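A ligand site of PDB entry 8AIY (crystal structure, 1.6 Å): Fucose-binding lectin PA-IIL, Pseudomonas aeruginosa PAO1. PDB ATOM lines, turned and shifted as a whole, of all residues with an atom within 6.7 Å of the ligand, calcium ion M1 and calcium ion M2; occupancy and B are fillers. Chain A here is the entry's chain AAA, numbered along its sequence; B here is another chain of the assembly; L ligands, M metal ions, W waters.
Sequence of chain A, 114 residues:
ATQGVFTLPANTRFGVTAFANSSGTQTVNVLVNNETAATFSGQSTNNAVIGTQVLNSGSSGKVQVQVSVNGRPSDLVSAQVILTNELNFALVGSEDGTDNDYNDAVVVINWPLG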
ATOM      1  N   ASN A  21       7.369  12.497  21.533  1.00  0.00           N
ATOM      2  CA  ASN A  21       8.297  12.253  22.649  1.00  0.00           C
ATOM      3  C   ASN A  21       8.473  13.541  23.444  1.00  0.00           C
ATOM      4  O   ASN A  21       9.528  14.183  23.343  1.00  0.00           O
ATOM      5  CB  ASN A  21       9.667  11.771  22.158  1.00  0.00           C
ATOM      6  CG  ASN A  21       9.568  10.397  21.554  1.00  0.00           C
ATOM      7  OD1 ASN A  21       9.585   9.404  22.260  1.00  0.00           O
ATOM      8  ND2 ASN A  21       9.572  10.355  20.234  1.00  0.00           N
ATOM      9  N   SER A  22       7.428  13.994  24.118  1.00  0.00           N
ATOM     10  CA  SER A  22       7.452  15.276  24.842  1.00  0.00           C
ATOM     11  C   SER A  22       6.328  15.271  25.864  1.00  0.00           C
ATOM     12  O   SER A  22       5.300  14.685  25.608  1.00  0.00           O
ATOM     13  CB  SER A  22       7.314  16.413  23.863  1.00  0.00           C
ATOM     14  OG  SER A  22       7.180  17.713  24.538  1.00  0.00           O
ATOM     15  N   SER A  23       6.505  16.070  26.927  1.00  0.00           N
ATOM     16  CA  SER A  23       5.400  16.335  27.881  1.00  0.00           C
ATOM     17  C   SER A  23       4.301  17.158  27.191  1.00  0.00           C
ATOM     18  O   SER A  23       3.127  17.112  27.693  1.00  0.00           O
ATOM     19  CB  SER A  23       5.920  17.031  29.092  1.00  0.00           C
ATOM     20  OG  SER A  23       6.564  18.256  28.740  1.00  0.00           O
ATOM     21  N   GLY A  24       4.583  17.878  26.137  1.00  0.00           N
ATOM     22  CA  GLY A  24       3.588  18.675  25.444  1.00  0.00           C
ATOM     23  C   GLY A  24       2.890  17.936  24.333  1.00  0.00           C
ATOM     24  O   GLY A  24       3.528  17.217  23.609  1.00  0.00           O
ATOM     25  N   THR A  25       1.614  18.187  24.162  1.00  0.00           N
ATOM     26  CA  THR A  25       0.850  17.733  22.982  1.00  0.00           C
ATOM     27  C   THR A  25       1.461  18.310  21.715  1.00  0.00           C
ATOM     28  O   THR A  25       1.673  19.525  21.598  1.00  0.00           O
ATOM     29  CB  THR A  25      -0.639  18.094  23.079  1.00  0.00           C
ATOM     30  OG1 THR A  25      -1.120  17.455  24.260  1.00  0.00           O
ATOM     31  CG2 THR A  25      -1.414  17.630  21.879  1.00  0.00           C
ATOM     32  N   GLN A  26       1.789  17.436  20.746  1.00  0.00           N
ATOM     33  CA  GLN A  26       2.327  17.877  19.447  1.00  0.00           C
ATOM     34  C   GLN A  26       1.216  18.001  18.433  1.00  0.00           C
ATOM     35  O   GLN A  26       0.326  17.105  18.400  1.00  0.00           O
ATOM     36  CB  GLN A  26       3.350  16.849  18.955  1.00  0.00           C
ATOM     37  CG  GLN A  26       4.371  16.446  19.994  1.00  0.00           C
ATOM     38  CD  GLN A  26       5.343  17.570  20.228  1.00  0.00           C
ATOM     39  OE1 GLN A  26       5.903  18.089  19.266  1.00  0.00           O
ATOM     40  NE2 GLN A  26       5.540  17.946  21.484  1.00  0.00           N
ATOM     41  N   SER A  44       2.735  11.993  23.858  1.00  0.00           N
ATOM     42  CA  SER A  44       3.431  10.805  24.331  1.00  0.00           C
ATOM     43  C   SER A  44       4.839  11.186  24.768  1.00  0.00           C
ATOM     44  O   SER A  44       5.421  12.025  24.089  1.00  0.00           O
ATOM     45  CB  SER A  44       3.490   9.746  23.214  1.00  0.00           C
ATOM     46  OG  SER A  44       4.103   8.559  23.691  1.00  0.00           O
ATOM     47  N   THR A  45       5.378  10.500  25.756  1.00  0.00           N
ATOM     48  CA  THR A  45       6.819  10.495  26.050  1.00  0.00           C
ATOM     49  C   THR A  45       7.418   9.143  25.682  1.00  0.00           C
ATOM     50  O   THR A  45       8.542   8.863  26.127  1.00  0.00           O
ATOM     51  CB  THR A  45       7.099  10.920  27.502  1.00  0.00           C
ATOM     52  OG1 THR A  45       6.234  10.121  28.348  1.00  0.00           O
ATOM     53  CG2 THR A  45       6.873  12.376  27.742  1.00  0.00           C
ATOM     54  N   VAL A  69       3.486  23.279  19.260  1.00  0.00           N
ATOM     55  CA  VAL A  69       3.256  22.817  20.639  1.00  0.00           C
ATOM     56  C   VAL A  69       2.757  24.033  21.408  1.00  0.00           C
ATOM     57  O   VAL A  69       3.395  25.075  21.338  1.00  0.00           O
ATOM     58  CB  VAL A  69       4.504  22.233  21.306  1.00  0.00           C
ATOM     59  CG1 VAL A  69       4.185  21.714  22.704  1.00  0.00           C
ATOM     60  CG2 VAL A  69       5.105  21.083  20.457  1.00  0.00           C
ATOM     61  N   ASN A  70       1.600  23.900  22.052  1.00  0.00           N
ATOM     62  CA  ASN A  70       1.035  25.059  22.810  1.00  0.00           C
ATOM     63  C   ASN A  70       0.926  26.279  21.906  1.00  0.00           C
ATOM     64  O   ASN A  70       1.106  27.419  22.390  1.00  0.00           O
ATOM     65  CB  ASN A  70       1.776  25.317  24.111  1.00  0.00           C
ATOM     66  CG  ASN A  70       1.386  24.411  25.260  1.00  0.00           C
ATOM     67  OD1 ASN A  70       0.603  23.493  25.075  1.00  0.00           O
ATOM     68  ND2 ASN A  70       1.910  24.710  26.465  1.00  0.00           N
ATOM     69  N   ARG A  72       2.799  27.201  19.368  1.00  0.00           N
ATOM     70  CA  ARG A  72       4.083  27.809  18.951  1.00  0.00           C
ATOM     71  C   ARG A  72       4.825  26.853  18.029  1.00  0.00           C
ATOM     72  O   ARG A  72       4.933  25.678  18.332  1.00  0.00           O
ATOM     73  CB  ARG A  72       4.926  28.053  20.186  1.00  0.00           C
ATOM     74  CG  ARG A  72       4.247  28.982  21.199  1.00  0.00           C
ATOM     75  CD  ARG A  72       5.164  29.440  22.311  1.00  0.00           C
ATOM     76  NE  ARG A  72       4.390  30.194  23.325  1.00  0.00           N
ATOM     77  CZ  ARG A  72       3.745  29.633  24.361  1.00  0.00           C
ATOM     78  NH1 ARG A  72       3.897  28.349  24.603  1.00  0.00           N
ATOM     79  NH2 ARG A  72       3.009  30.397  25.168  1.00  0.00           N
ATOM     80  N   SER A  94      11.959  17.635  15.532  1.00  0.00           N
ATOM     81  CA  SER A  94      11.425  18.940  15.981  1.00  0.00           C
ATOM     82  C   SER A  94      11.742  19.104  17.439  1.00  0.00           C
ATOM     83  O   SER A  94      11.723  18.098  18.187  1.00  0.00           O
ATOM     84  CB  SER A  94       9.990  19.082  15.659  1.00  0.00           C
ATOM     85  OG  SER A  94       9.165  18.183  16.391  1.00  0.00           O
ATOM     86  N   GLU A  95      11.992  20.346  17.831  1.00  0.00           N
ATOM     87  CA  GLU A  95      12.352  20.680  19.228  1.00  0.00           C
ATOM     88  C   GLU A  95      11.369  21.757  19.744  1.00  0.00           C
ATOM     89  O   GLU A  95      11.243  22.804  19.113  1.00  0.00           O
ATOM     90  CB  GLU A  95      13.783  21.223  19.306  1.00  0.00           C
ATOM     91  CG  GLU A  95      14.146  21.589  20.721  1.00  0.00           C
ATOM     92  CD  GLU A  95      13.944  20.470  21.727  1.00  0.00           C
ATOM     93  OE1 GLU A  95      14.381  19.319  21.478  1.00  0.00           O
ATOM     94  OE2 GLU A  95      13.296  20.736  22.794  1.00  0.00           O
ATOM     95  N   ASP A  96      10.685  21.437  20.821  1.00  0.00           N
ATOM     96  CA  ASP A  96       9.694  22.357  21.413  1.00  0.00           C
ATOM     97  C   ASP A  96      10.222  23.054  22.661  1.00  0.00           C
ATOM     98  O   ASP A  96       9.444  23.871  23.197  1.00  0.00           O
ATOM     99  CB  ASP A  96       8.422  21.551  21.736  1.00  0.00           C
ATOM    100  CG  ASP A  96       8.584  20.438  22.746  1.00  0.00           C
ATOM    101  OD1 ASP A  96       9.517  20.454  23.540  1.00  0.00           O
ATOM    102  OD2 ASP A  96       7.661  19.521  22.808  1.00  0.00           O
ATOM    103  N   GLY A  97      11.424  22.740  23.116  1.00  0.00           N
ATOM    104  CA  GLY A  97      11.935  23.230  24.399  1.00  0.00           C
ATOM    105  C   GLY A  97      13.434  23.463  24.348  1.00  0.00           C
ATOM    106  O   GLY A  97      13.887  24.122  23.404  1.00  0.00           O
ATOM    107  N   THR A  98      14.099  23.056  25.388  1.00  0.00           N
ATOM    108  CA  THR A  98      15.475  23.526  25.658  1.00  0.00           C
ATOM    109  C   THR A  98      16.491  22.398  25.597  1.00  0.00           C
ATOM    110  O   THR A  98      17.679  22.731  25.566  1.00  0.00           O
ATOM    111  CB  THR A  98      15.540  24.221  27.023  1.00  0.00           C
ATOM    112  OG1 THR A  98      15.130  23.296  28.019  1.00  0.00           O
ATOM    113  CG2 THR A  98      14.688  25.462  27.031  1.00  0.00           C
ATOM    114  N   ASP A  99      16.099  21.119  25.570  1.00  0.00           N
ATOM    115  CA  ASP A  99      17.051  20.014  25.692  1.00  0.00           C
ATOM    116  C   ASP A  99      17.668  19.609  24.335  1.00  0.00           C
ATOM    117  O   ASP A  99      18.621  18.847  24.365  1.00  0.00           O
ATOM    118  CB  ASP A  99      16.445  18.828  26.410  1.00  0.00           C
ATOM    119  CG  ASP A  99      15.350  18.115  25.641  1.00  0.00           C
ATOM    120  OD1 ASP A  99      14.865  18.724  24.647  1.00  0.00           O
ATOM    121  OD2 ASP A  99      15.019  16.987  26.092  1.00  0.00           O
ATOM    122  N   ASN A 100      17.158  20.126  23.239  1.00  0.00           N
ATOM    123  CA  ASN A 100      17.708  19.827  21.889  1.00  0.00           C
ATOM    124  C   ASN A 100      17.806  18.332  21.633  1.00  0.00           C
ATOM    125  O   ASN A 100      18.748  17.886  20.952  1.00  0.00           O
ATOM    126  CB  ASN A 100      19.030  20.571  21.693  1.00  0.00           C
ATOM    127  CG  ASN A 100      18.787  22.051  21.735  1.00  0.00           C
ATOM    128  OD1 ASN A 100      17.685  22.540  21.431  1.00  0.00           O
ATOM    129  ND2 ASN A 100      19.788  22.796  22.129  1.00  0.00           N
ATOM    130  N   ASP A 101      16.821  17.552  22.070  1.00  0.00           N
ATOM    131  CA  ASP A 101      16.754  16.151  21.632  1.00  0.00           C
ATOM    132  C   ASP A 101      16.116  16.063  20.238  1.00  0.00           C
ATOM    133  O   ASP A 101      16.349  15.031  19.579  1.00  0.00           O
ATOM    134  CB  ASP A 101      16.122  15.240  22.678  1.00  0.00           C
ATOM    135  CG  ASP A 101      14.675  15.487  23.047  1.00  0.00           C
ATOM    136  OD1 ASP A 101      14.094  16.454  22.527  1.00  0.00           O
ATOM    137  OD2 ASP A 101      14.163  14.599  23.820  1.00  0.00           O
ATOM    138  N   TYR A 102      15.363  17.059  19.799  1.00  0.00           N
ATOM    139  CA  TYR A 102      14.771  17.118  18.436  1.00  0.00           C
ATOM    140  C   TYR A 102      13.924  15.879  18.145  1.00  0.00           C
ATOM    141  O   TYR A 102      13.645  15.611  16.987  1.00  0.00           O
ATOM    142  CB  TYR A 102      15.882  17.348  17.382  1.00  0.00           C
ATOM    143  CG  TYR A 102      16.179  18.831  17.290  1.00  0.00           C
ATOM    144  CD1 TYR A 102      15.502  19.642  16.432  1.00  0.00           C
ATOM    145  CD2 TYR A 102      17.109  19.391  18.148  1.00  0.00           C
ATOM    146  CE1 TYR A 102      15.691  21.025  16.436  1.00  0.00           C
ATOM    147  CE2 TYR A 102      17.340  20.764  18.144  1.00  0.00           C
ATOM    148  CZ  TYR A 102      16.624  21.573  17.299  1.00  0.00           C
ATOM    149  OH  TYR A 102      16.746  22.914  17.311  1.00  0.00           O
ATOM    150  N   ASN A 103      13.339  15.234  19.172  1.00  0.00           N
ATOM    151  CA  ASN A 103      12.464  14.046  18.983  1.00  0.00           C
ATOM    152  C   ASN A 103      11.041  14.382  19.405  1.00  0.00           C
ATOM    153  O   ASN A 103      10.238  13.464  19.483  1.00  0.00           O
ATOM    154  CB  ASN A 103      12.998  12.844  19.713  1.00  0.00           C
ATOM    155  CG  ASN A 103      12.770  12.943  21.211  1.00  0.00           C
ATOM    156  OD1 ASN A 103      12.331  13.998  21.685  1.00  0.00           O
ATOM    157  ND2 ASN A 103      13.156  11.930  21.930  1.00  0.00           N
ATOM    158  N   ASP A 104      10.734  15.642  19.684  1.00  0.00           N
ATOM    159  CA  ASP A 104       9.481  15.965  20.392  1.00  0.00           C
ATOM    160  C   ASP A 104       8.309  15.585  19.509  1.00  0.00           C
ATOM    161  O   ASP A 104       7.349  14.978  20.033  1.00  0.00           O
ATOM    162  CB  ASP A 104       9.525  17.424  20.834  1.00  0.00           C
ATOM    163  CG  ASP A 104      10.662  17.693  21.788  1.00  0.00           C
ATOM    164  OD1 ASP A 104      10.982  16.815  22.623  1.00  0.00           O
ATOM    165  OD2 ASP A 104      11.264  18.780  21.653  1.00  0.00           O
ATOM    166  N   ALA A 105       8.355  15.902  18.231  1.00  0.00           N
ATOM    167  CA  ALA A 105       7.618  15.202  17.178  1.00  0.00           C
ATOM    168  C   ALA A 105       8.653  14.723  16.175  1.00  0.00           C
ATOM    169  O   ALA A 105       9.508  15.557  15.727  1.00  0.00           O
ATOM    170  CB  ALA A 105       6.563  16.062  16.518  1.00  0.00           C
ATOM    171  N   PRO B 112      17.094   9.091  20.175  1.00  0.00           N
ATOM    172  CA  PRO B 112      16.510   8.645  21.426  1.00  0.00           C
ATOM    173  C   PRO B 112      15.010   8.977  21.494  1.00  0.00           C
ATOM    174  O   PRO B 112      14.445   9.727  20.697  1.00  0.00           O
ATOM    175  CB  PRO B 112      17.232   9.526  22.435  1.00  0.00           C
ATOM    176  CG  PRO B 112      17.444  10.825  21.679  1.00  0.00           C
ATOM    177  CD  PRO B 112      17.801  10.370  20.272  1.00  0.00           C
ATOM    178  N   LEU B 113      14.394   8.371  22.501  1.00  0.00           N
ATOM    179  CA  LEU B 113      12.984   8.595  22.830  1.00  0.00           C
ATOM    180  C   LEU B 113      12.865   9.518  24.046  1.00  0.00           C
ATOM    181  O   LEU B 113      13.847   9.899  24.644  1.00  0.00           O
ATOM    182  CB  LEU B 113      12.299   7.273  23.098  1.00  0.00           C
ATOM    183  CG  LEU B 113      12.457   6.198  22.005  1.00  0.00           C
ATOM    184  CD1 LEU B 113      11.535   4.994  22.318  1.00  0.00           C
ATOM    185  CD2 LEU B 113      12.097   6.759  20.653  1.00  0.00           C
ATOM    186  N   GLY B 114      11.630   9.827  24.403  1.00  0.00           N
ATOM    187  CA  GLY B 114      11.334  10.561  25.662  1.00  0.00           C
ATOM    188  C   GLY B 114      11.341  12.054  25.511  1.00  0.00           C
ATOM    189  O   GLY B 114      11.891  12.670  24.565  1.00  0.00           O
ATOM    190  OXT GLY B 114      10.713  12.648  26.458  1.00  0.00           O
HETATM  191  C1  LIG L   1       9.611  15.308  28.710  1.00  0.00           C
HETATM  192  C2  LIG L   1      10.277  16.473  28.006  1.00  0.00           C
HETATM  193  C3  LIG L   1      11.285  16.041  26.942  1.00  0.00           C
HETATM  194  C4  LIG L   1      11.859  17.217  26.176  1.00  0.00           C
HETATM  195  C5  LIG L   1      10.711  18.037  25.659  1.00  0.00           C
HETATM  196  C6  LIG L   1       9.822  18.470  26.821  1.00  0.00           C
HETATM  197  O1  LIG L   1       9.276  17.299  27.409  1.00  0.00           O
HETATM  198  O2  LIG L   1      11.285  19.096  24.912  1.00  0.00           O
HETATM  199  O3  LIG L   1      12.668  16.774  25.049  1.00  0.00           O
HETATM  200  O4  LIG L   1      10.725  15.150  25.940  1.00  0.00           O
HETATM  201  N1  LIG L   1       8.741  19.294  26.413  1.00  0.00           N
HETATM  202  C7  LIG L   1       8.742  20.625  26.555  1.00  0.00           C
HETATM  203  O5  LIG L   1       9.767  21.248  26.865  1.00  0.00           O
HETATM  204  C8  LIG L   1       7.469  21.349  26.306  1.00  0.00           C
HETATM  205  C9  LIG L   1       7.428  22.450  25.457  1.00  0.00           C
HETATM  206  C10 LIG L   1       6.277  23.161  25.286  1.00  0.00           C
HETATM  207  C11 LIG L   1       5.139  22.818  26.018  1.00  0.00           C
HETATM  208  C12 LIG L   1       5.156  21.713  26.848  1.00  0.00           C
HETATM  209  C13 LIG L   1       3.970  21.349  27.685  1.00  0.00           C
HETATM  210  C14 LIG L   1       2.672  21.609  27.260  1.00  0.00           C
HETATM  211  C15 LIG L   1       1.579  21.351  28.083  1.00  0.00           C
HETATM  212  C16 LIG L   1       1.793  20.777  29.303  1.00  0.00           C
HETATM  213  C17 LIG L   1       3.069  20.560  29.769  1.00  0.00           C
HETATM  214  C18 LIG L   1       4.150  20.847  28.948  1.00  0.00           C
HETATM  215  C19 LIG L   1       6.320  20.995  26.995  1.00  0.00           C
HETATM  216 CA    CA M   1      11.760  14.890  23.746  1.00  0.00          CA
HETATM  217 CA    CA M   2      12.994  18.386  23.261  1.00  0.00          CA
HETATM  218  O   HOH W   1      13.068  20.693  26.579  1.00  0.00           O
HETATM  219  O   HOH W   2      10.048  23.865  27.477  1.00  0.00           O
HETATM  220  O   HOH W   3       9.253  25.392  25.509  1.00  0.00           O
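Calcium ion M1 is bound by OD1 of Asn 103, OD1 of Asp 104, O of Gly 114 of chain B, O of Asn 21, OD2 of Asp 101, O4 of the ligand and O3 of the ligand. Slightly farther from calcium ion M1 lies OD1 of Asp 101 (3.1 Å).
Calcium ion M2 is bound by OD1 of Asp 101 (2.3 Å), OD1 of Asp 99 (2.4 Å), OD2 of Asp 104 (2.4 Å), OE2 of Glu 95 (2.4 Å), O3 of the ligand (2.4 Å), OE1 of Glu 95 (2.4 Å), O2 of the ligand (2.5 Å) and OD1 of Asp 104 (2.6 Å).
CA of Gly 24 touches C13 of the ligand (3.5 Å). CG1 of Val 69 touches C11 of the ligand, at 3.6 Å. Asn 70 touches the ligand. Gly 97 touches the ligand (CA to O5, 3.8 Å). Hydrophobic or aromatic side chains within 4 Å of the ligand: Val 69. 13 residues have an atom within 4 Å of the ligand: Asn 21, Ser 22, Ser 23, Gly 24, Val 69, Asn 70, Glu 95, Asp 96, Gly 97, Asp 99, Asp 101, Asp 104 and Gly 114 of chain B.
Water W1 lies within hydrogen-bond range of N of Thr 98, N of Asp 99 and O5 of the ligand.
Within 4 Å of calcium ion M1: Asn 21, Asp 101, Asn 103, Asp 104 and Gly 114 of chain B. The nearest printed residue that does not touch calcium ion M1 is Ser 22 (4.4 Å).
The side-chain carboxylate (OD1) of Asp 96 sits close to a nitrogen (N1) of the ligand, 3.2 Å away. OG of Ser 22 lies within hydrogen-bond range of N1 of the ligand, 2.9 Å away. The backbone NH of Ser 23 is in hydrogen-bond range of an oxygen (O1) of the ligand, 3.1 Å away. The side-chain hydroxyl of Ser 23 is in hydrogen-bond range of an oxygen (O1) of the ligand.
N of Asp 96 sits close to OD2 of Asp 104 (2.8 Å). The backbone NH of Asp 104 sits at hydrogen-bond distance from the backbone carbonyl oxygen of Ser 94, at 3.0 Å. The backbone NH (N) of Asn 21 sits close to the backbone carbonyl oxygen (O) of Ser 44 (3.2 Å). N of Gly 97 lies close to OE2 of Glu 95 (2.8 Å). The side-chain carboxylate (OE1) of Glu 95 lies close to the backbone NH (N) of Tyr 102. The backbone NH (N) of Gly 24 sits at hydrogen-bond distance from the side-chain hydroxyl (OG) of Ser 22, 3.1 Å away. The backbone carbonyl oxygen (O) of Ser 44 is in hydrogen-bond range of the backbone NH (N) of Ser 22 (2.8 Å). O of Gly 24 lies within hydrogen-bond range of NE2 of Gln 26 (3.0 Å).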
